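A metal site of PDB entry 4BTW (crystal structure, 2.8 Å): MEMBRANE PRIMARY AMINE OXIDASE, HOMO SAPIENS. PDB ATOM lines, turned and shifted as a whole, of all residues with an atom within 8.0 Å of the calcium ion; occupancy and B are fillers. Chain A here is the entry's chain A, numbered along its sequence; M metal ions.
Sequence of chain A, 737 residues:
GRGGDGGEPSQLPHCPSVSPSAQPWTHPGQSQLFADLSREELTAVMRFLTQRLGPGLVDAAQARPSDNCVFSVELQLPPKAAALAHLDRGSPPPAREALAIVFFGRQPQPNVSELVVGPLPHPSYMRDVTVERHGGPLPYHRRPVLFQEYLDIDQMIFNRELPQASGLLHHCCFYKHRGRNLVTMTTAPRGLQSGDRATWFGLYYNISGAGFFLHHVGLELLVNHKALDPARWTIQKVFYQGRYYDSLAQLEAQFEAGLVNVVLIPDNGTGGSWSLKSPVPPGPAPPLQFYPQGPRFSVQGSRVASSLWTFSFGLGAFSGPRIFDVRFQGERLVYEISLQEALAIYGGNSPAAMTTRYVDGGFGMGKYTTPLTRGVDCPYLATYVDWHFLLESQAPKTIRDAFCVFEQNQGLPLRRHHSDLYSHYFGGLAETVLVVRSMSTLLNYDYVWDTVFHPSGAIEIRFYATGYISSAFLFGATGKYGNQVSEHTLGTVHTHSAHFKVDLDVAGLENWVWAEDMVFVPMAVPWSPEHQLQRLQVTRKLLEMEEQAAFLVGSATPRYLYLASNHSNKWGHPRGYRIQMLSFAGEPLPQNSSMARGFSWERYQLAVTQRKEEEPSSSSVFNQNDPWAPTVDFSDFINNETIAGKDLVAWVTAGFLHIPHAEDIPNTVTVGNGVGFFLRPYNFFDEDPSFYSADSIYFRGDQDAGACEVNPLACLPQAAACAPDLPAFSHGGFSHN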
ATOM      1  N   GLU A 546      -9.597  24.950  -3.754  1.00  0.00           N
ATOM      2  CA  GLU A 546      -9.134  24.787  -2.365  1.00  0.00           C
ATOM      3  C   GLU A 546      -7.576  25.082  -2.292  1.00  0.00           C
ATOM      4  O   GLU A 546      -7.099  25.915  -1.460  1.00  0.00           O
ATOM      5  CB  GLU A 546      -9.613  23.396  -1.780  1.00  0.00           C
ATOM      6  CG  GLU A 546     -11.070  23.369  -1.280  1.00  0.00           C
ATOM      7  CD  GLU A 546     -11.541  22.077  -0.583  1.00  0.00           C
ATOM      8  OE1 GLU A 546     -11.072  20.966  -0.906  1.00  0.00           O
ATOM      9  OE2 GLU A 546     -12.438  22.124   0.312  1.00  0.00           O
ATOM     10  N   GLU A 547      -6.823  24.495  -3.231  1.00  0.00           N
ATOM     11  CA  GLU A 547      -5.352  24.573  -3.204  1.00  0.00           C
ATOM     12  C   GLU A 547      -4.822  25.984  -3.417  1.00  0.00           C
ATOM     13  O   GLU A 547      -3.804  26.379  -2.847  1.00  0.00           O
ATOM     14  CB  GLU A 547      -4.664  23.559  -4.122  1.00  0.00           C
ATOM     15  CG  GLU A 547      -5.525  22.903  -5.188  1.00  0.00           C
ATOM     16  CD  GLU A 547      -6.369  21.763  -4.642  1.00  0.00           C
ATOM     17  OE1 GLU A 547      -5.846  20.976  -3.805  1.00  0.00           O
ATOM     18  OE2 GLU A 547      -7.548  21.656  -5.061  1.00  0.00           O
ATOM     19  N   VAL A 608      -8.560  27.447   3.036  1.00  0.00           N
ATOM     20  CA  VAL A 608      -9.998  27.538   2.965  1.00  0.00           C
ATOM     21  C   VAL A 608     -10.578  26.355   2.193  1.00  0.00           C
ATOM     22  O   VAL A 608     -10.104  25.979   1.102  1.00  0.00           O
ATOM     23  CB  VAL A 608     -10.445  28.869   2.386  1.00  0.00           C
ATOM     24  CG1 VAL A 608     -11.948  28.944   2.470  1.00  0.00           C
ATOM     25  CG2 VAL A 608      -9.839  30.011   3.175  1.00  0.00           C
ATOM     26  N   THR A 609     -11.577  25.736   2.795  1.00  0.00           N
ATOM     27  CA  THR A 609     -12.153  24.544   2.234  1.00  0.00           C
ATOM     28  C   THR A 609     -13.646  24.688   2.183  1.00  0.00           C
ATOM     29  O   THR A 609     -14.243  25.593   2.828  1.00  0.00           O
ATOM     30  CB  THR A 609     -11.816  23.322   3.082  1.00  0.00           C
ATOM     31  OG1 THR A 609     -11.924  23.674   4.461  1.00  0.00           O
ATOM     32  CG2 THR A 609     -10.424  22.885   2.821  1.00  0.00           C
ATOM     33  N   GLN A 610     -14.233  23.789   1.380  1.00  0.00           N
ATOM     34  CA  GLN A 610     -15.662  23.490   1.419  1.00  0.00           C
ATOM     35  C   GLN A 610     -16.009  22.890   2.764  1.00  0.00           C
ATOM     36  O   GLN A 610     -15.440  21.830   3.145  1.00  0.00           O
ATOM     37  CB  GLN A 610     -16.010  22.477   0.362  1.00  0.00           C
ATOM     38  CG  GLN A 610     -16.454  23.098  -0.931  1.00  0.00           C
ATOM     39  CD  GLN A 610     -16.934  22.056  -1.904  1.00  0.00           C
ATOM     40  OE1 GLN A 610     -17.364  20.981  -1.508  1.00  0.00           O
ATOM     41  NE2 GLN A 610     -16.867  22.383  -3.174  1.00  0.00           N
ATOM     42  N   ARG A 611     -16.939  23.569   3.454  1.00  0.00           N
ATOM     43  CA  ARG A 611     -17.277  23.261   4.838  1.00  0.00           C
ATOM     44  C   ARG A 611     -18.139  22.045   4.817  1.00  0.00           C
ATOM     45  O   ARG A 611     -19.042  21.963   4.036  1.00  0.00           O
ATOM     46  CB  ARG A 611     -18.018  24.430   5.504  1.00  0.00           C
ATOM     47  CG  ARG A 611     -18.579  24.085   6.872  1.00  0.00           C
ATOM     48  CD  ARG A 611     -20.059  23.748   6.767  1.00  0.00           C
ATOM     49  NE  ARG A 611     -20.607  22.805   7.745  1.00  0.00           N
ATOM     50  CZ  ARG A 611     -20.674  23.009   9.066  1.00  0.00           C
ATOM     51  NH1 ARG A 611     -20.143  24.110   9.633  1.00  0.00           N
ATOM     52  NH2 ARG A 611     -21.252  22.071   9.812  1.00  0.00           N
ATOM     53  N   LYS A 612     -17.864  21.081   5.691  1.00  0.00           N
ATOM     54  CA  LYS A 612     -18.614  19.824   5.623  1.00  0.00           C
ATOM     55  C   LYS A 612     -19.031  19.228   6.966  1.00  0.00           C
ATOM     56  O   LYS A 612     -18.492  19.574   8.064  1.00  0.00           O
ATOM     57  CB  LYS A 612     -17.836  18.771   4.846  1.00  0.00           C
ATOM     58  CG  LYS A 612     -17.496  19.163   3.418  1.00  0.00           C
ATOM     59  CD  LYS A 612     -16.828  17.963   2.752  1.00  0.00           C
ATOM     60  CE  LYS A 612     -17.058  17.864   1.257  1.00  0.00           C
ATOM     61  NZ  LYS A 612     -15.856  18.288   0.510  1.00  0.00           N
ATOM     62  N   GLU A 615     -16.362  17.004   7.740  1.00  0.00           N
ATOM     63  CA  GLU A 615     -15.113  17.712   8.042  1.00  0.00           C
ATOM     64  C   GLU A 615     -15.399  18.689   9.178  1.00  0.00           C
ATOM     65  O   GLU A 615     -15.461  19.899   8.975  1.00  0.00           O
ATOM     66  CB  GLU A 615     -14.517  18.363   6.776  1.00  0.00           C
ATOM     67  CG  GLU A 615     -14.113  17.301   5.748  1.00  0.00           C
ATOM     68  CD  GLU A 615     -13.635  17.833   4.404  1.00  0.00           C
ATOM     69  OE1 GLU A 615     -13.685  19.081   4.060  1.00  0.00           O
ATOM     70  OE2 GLU A 615     -13.213  16.913   3.672  1.00  0.00           O
ATOM     71  N   PHE A 634      -5.611  16.735   8.371  1.00  0.00           N
ATOM     72  CA  PHE A 634      -6.269  17.936   7.853  1.00  0.00           C
ATOM     73  C   PHE A 634      -5.978  18.218   6.405  1.00  0.00           C
ATOM     74  O   PHE A 634      -6.719  18.972   5.759  1.00  0.00           O
ATOM     75  CB  PHE A 634      -5.848  19.110   8.691  1.00  0.00           C
ATOM     76  CG  PHE A 634      -6.214  20.445   8.120  1.00  0.00           C
ATOM     77  CD1 PHE A 634      -5.342  21.113   7.314  1.00  0.00           C
ATOM     78  CD2 PHE A 634      -7.389  21.048   8.477  1.00  0.00           C
ATOM     79  CE1 PHE A 634      -5.649  22.363   6.838  1.00  0.00           C
ATOM     80  CE2 PHE A 634      -7.695  22.290   7.996  1.00  0.00           C
ATOM     81  CZ  PHE A 634      -6.833  22.945   7.190  1.00  0.00           C
ATOM     82  N   SER A 635      -4.893  17.644   5.902  1.00  0.00           N
ATOM     83  CA  SER A 635      -4.522  17.761   4.491  1.00  0.00           C
ATOM     84  C   SER A 635      -5.514  17.038   3.593  1.00  0.00           C
ATOM     85  O   SER A 635      -5.504  17.274   2.386  1.00  0.00           O
ATOM     86  CB  SER A 635      -3.094  17.247   4.250  1.00  0.00           C
ATOM     87  OG  SER A 635      -3.025  15.827   4.217  1.00  0.00           O
ATOM     88  N   ASP A 636      -6.344  16.161   4.149  1.00  0.00           N
ATOM     89  CA  ASP A 636      -7.400  15.519   3.357  1.00  0.00           C
ATOM     90  C   ASP A 636      -8.510  16.496   2.916  1.00  0.00           C
ATOM     91  O   ASP A 636      -9.167  16.314   1.856  1.00  0.00           O
ATOM     92  CB  ASP A 636      -8.071  14.400   4.137  1.00  0.00           C
ATOM     93  CG  ASP A 636      -7.149  13.282   4.445  1.00  0.00           C
ATOM     94  OD1 ASP A 636      -6.182  13.094   3.684  1.00  0.00           O
ATOM     95  OD2 ASP A 636      -7.434  12.591   5.462  1.00  0.00           O
ATOM     96  N   PHE A 637      -8.703  17.521   3.731  1.00  0.00           N
ATOM     97  CA  PHE A 637      -9.755  18.482   3.486  1.00  0.00           C
ATOM     98  C   PHE A 637      -9.472  19.288   2.216  1.00  0.00           C
ATOM     99  O   PHE A 637     -10.371  19.909   1.667  1.00  0.00           O
ATOM    100  CB  PHE A 637      -9.844  19.495   4.618  1.00  0.00           C
ATOM    101  CG  PHE A 637     -10.220  18.918   5.959  1.00  0.00           C
ATOM    102  CD1 PHE A 637     -10.193  17.547   6.210  1.00  0.00           C
ATOM    103  CD2 PHE A 637     -10.576  19.810   6.989  1.00  0.00           C
ATOM    104  CE1 PHE A 637     -10.533  17.081   7.448  1.00  0.00           C
ATOM    105  CE2 PHE A 637     -10.918  19.338   8.235  1.00  0.00           C
ATOM    106  CZ  PHE A 637     -10.886  17.969   8.465  1.00  0.00           C
ATOM    107  N   ILE A 638      -8.201  19.299   1.806  1.00  0.00           N
ATOM    108  CA  ILE A 638      -7.751  20.054   0.653  1.00  0.00           C
ATOM    109  C   ILE A 638      -7.480  19.135  -0.545  1.00  0.00           C
ATOM    110  O   ILE A 638      -6.381  18.579  -0.699  1.00  0.00           O
ATOM    111  CB  ILE A 638      -6.520  20.857   1.047  1.00  0.00           C
ATOM    112  CG1 ILE A 638      -6.863  21.745   2.245  1.00  0.00           C
ATOM    113  CG2 ILE A 638      -6.076  21.690  -0.120  1.00  0.00           C
ATOM    114  CD1 ILE A 638      -5.963  22.945   2.457  1.00  0.00           C
ATOM    115  N   ASN A 639      -8.534  19.036  -1.385  1.00  0.00           N
ATOM    116  CA  ASN A 639      -8.685  18.132  -2.531  1.00  0.00           C
ATOM    117  C   ASN A 639      -9.185  18.972  -3.691  1.00  0.00           C
ATOM    118  O   ASN A 639      -9.730  20.052  -3.489  1.00  0.00           O
ATOM    119  CB  ASN A 639      -9.682  17.006  -2.217  1.00  0.00           C
ATOM    120  CG  ASN A 639     -11.018  17.488  -1.566  1.00  0.00           C
ATOM    121  OD1 ASN A 639     -11.112  18.448  -0.780  1.00  0.00           O
ATOM    122  ND2 ASN A 639     -12.052  16.757  -1.868  1.00  0.00           N
ATOM    123  N   ASN A 640      -9.010  18.518  -4.924  1.00  0.00           N
ATOM    124  CA  ASN A 640      -9.294  19.371  -6.085  1.00  0.00           C
ATOM    125  C   ASN A 640     -10.752  19.824  -6.080  1.00  0.00           C
ATOM    126  O   ASN A 640     -11.610  19.194  -6.697  1.00  0.00           O
ATOM    127  CB  ASN A 640      -8.933  18.645  -7.394  1.00  0.00           C
ATOM    128  CG  ASN A 640      -9.067  19.534  -8.628  1.00  0.00           C
ATOM    129  OD1 ASN A 640      -8.756  20.740  -8.576  1.00  0.00           O
ATOM    130  ND2 ASN A 640      -9.554  18.922  -9.758  1.00  0.00           N
ATOM    131  N   GLU A 641     -11.030  20.917  -5.376  1.00  0.00           N
ATOM    132  CA  GLU A 641     -12.416  21.338  -5.146  1.00  0.00           C
ATOM    133  C   GLU A 641     -12.593  22.812  -5.225  1.00  0.00           C
ATOM    134  O   GLU A 641     -11.776  23.528  -4.684  1.00  0.00           O
ATOM    135  CB  GLU A 641     -12.901  20.910  -3.763  1.00  0.00           C
ATOM    136  CG  GLU A 641     -13.576  19.539  -3.763  1.00  0.00           C
ATOM    137  CD  GLU A 641     -14.116  19.131  -2.404  1.00  0.00           C
ATOM    138  OE1 GLU A 641     -13.548  19.522  -1.380  1.00  0.00           O
ATOM    139  OE2 GLU A 641     -15.123  18.391  -2.370  1.00  0.00           O
ATOM    140  N   THR A 642     -13.674  23.255  -5.844  1.00  0.00           N
ATOM    141  CA  THR A 642     -13.973  24.682  -5.886  1.00  0.00           C
ATOM    142  C   THR A 642     -14.354  25.293  -4.543  1.00  0.00           C
ATOM    143  O   THR A 642     -14.904  24.632  -3.667  1.00  0.00           O
ATOM    144  CB  THR A 642     -15.139  25.012  -6.823  1.00  0.00           C
ATOM    145  OG1 THR A 642     -15.587  26.366  -6.573  1.00  0.00           O
ATOM    146  CG2 THR A 642     -16.296  24.029  -6.602  1.00  0.00           C
ATOM    147  N   ILE A 643     -14.053  26.594  -4.436  1.00  0.00           N
ATOM    148  CA  ILE A 643     -14.456  27.454  -3.341  1.00  0.00           C
ATOM    149  C   ILE A 643     -14.978  28.747  -3.950  1.00  0.00           C
ATOM    150  O   ILE A 643     -14.783  29.898  -3.432  1.00  0.00           O
ATOM    151  CB  ILE A 643     -13.278  27.706  -2.401  1.00  0.00           C
ATOM    152  CG1 ILE A 643     -12.037  28.164  -3.178  1.00  0.00           C
ATOM    153  CG2 ILE A 643     -12.953  26.423  -1.689  1.00  0.00           C
ATOM    154  CD1 ILE A 643     -10.799  28.428  -2.324  1.00  0.00           C
ATOM    155  N   TRP A 651      -9.366  28.105   7.951  1.00  0.00           N
ATOM    156  CA  TRP A 651      -8.643  27.394   8.955  1.00  0.00           C
ATOM    157  C   TRP A 651      -7.299  28.027   9.283  1.00  0.00           C
ATOM    158  O   TRP A 651      -6.265  27.701   8.668  1.00  0.00           O
ATOM    159  CB  TRP A 651      -8.378  26.022   8.423  1.00  0.00           C
ATOM    160  CG  TRP A 651      -9.533  25.190   8.054  1.00  0.00           C
ATOM    161  CD1 TRP A 651      -9.976  24.919   6.810  1.00  0.00           C
ATOM    162  CD2 TRP A 651     -10.322  24.373   8.932  1.00  0.00           C
ATOM    163  NE1 TRP A 651     -10.997  24.004   6.841  1.00  0.00           N
ATOM    164  CE2 TRP A 651     -11.224  23.645   8.136  1.00  0.00           C
ATOM    165  CE3 TRP A 651     -10.351  24.181  10.318  1.00  0.00           C
ATOM    166  CZ2 TRP A 651     -12.144  22.757   8.676  1.00  0.00           C
ATOM    167  CZ3 TRP A 651     -11.268  23.297  10.849  1.00  0.00           C
ATOM    168  CH2 TRP A 651     -12.144  22.599  10.029  1.00  0.00           C
HETATM  169 CA    CA M   1     -12.446  19.780   0.625  1.00  0.00          CA
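OE2 of Glu 641 is in salt-bridge range of NZ of Lys 612, 3.0 Å away. The side-chain carboxylate (OE2) of Glu 546 sits close to the backbone NH (N) of Gln 610 (2.7 Å).
Merely in contact with the calcium ion: Lys 612 (3.7 Å) and Glu 615 (3.7 Å). Along chain A the residues within 4 Å of the calcium ion span positions 546 to 641.
The calcium ion is bound by the side-chain carboxylate (OE1) of Glu 641, the backbone carbonyl oxygen (O) of Phe 637, the side-chain amide oxygen (OD1) of Asn 639, the side-chain carboxylate (OE2) of Glu 546 and the side-chain carboxylate (OE1) of Glu 546. The calcium ion has five donor atoms within binding distance.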
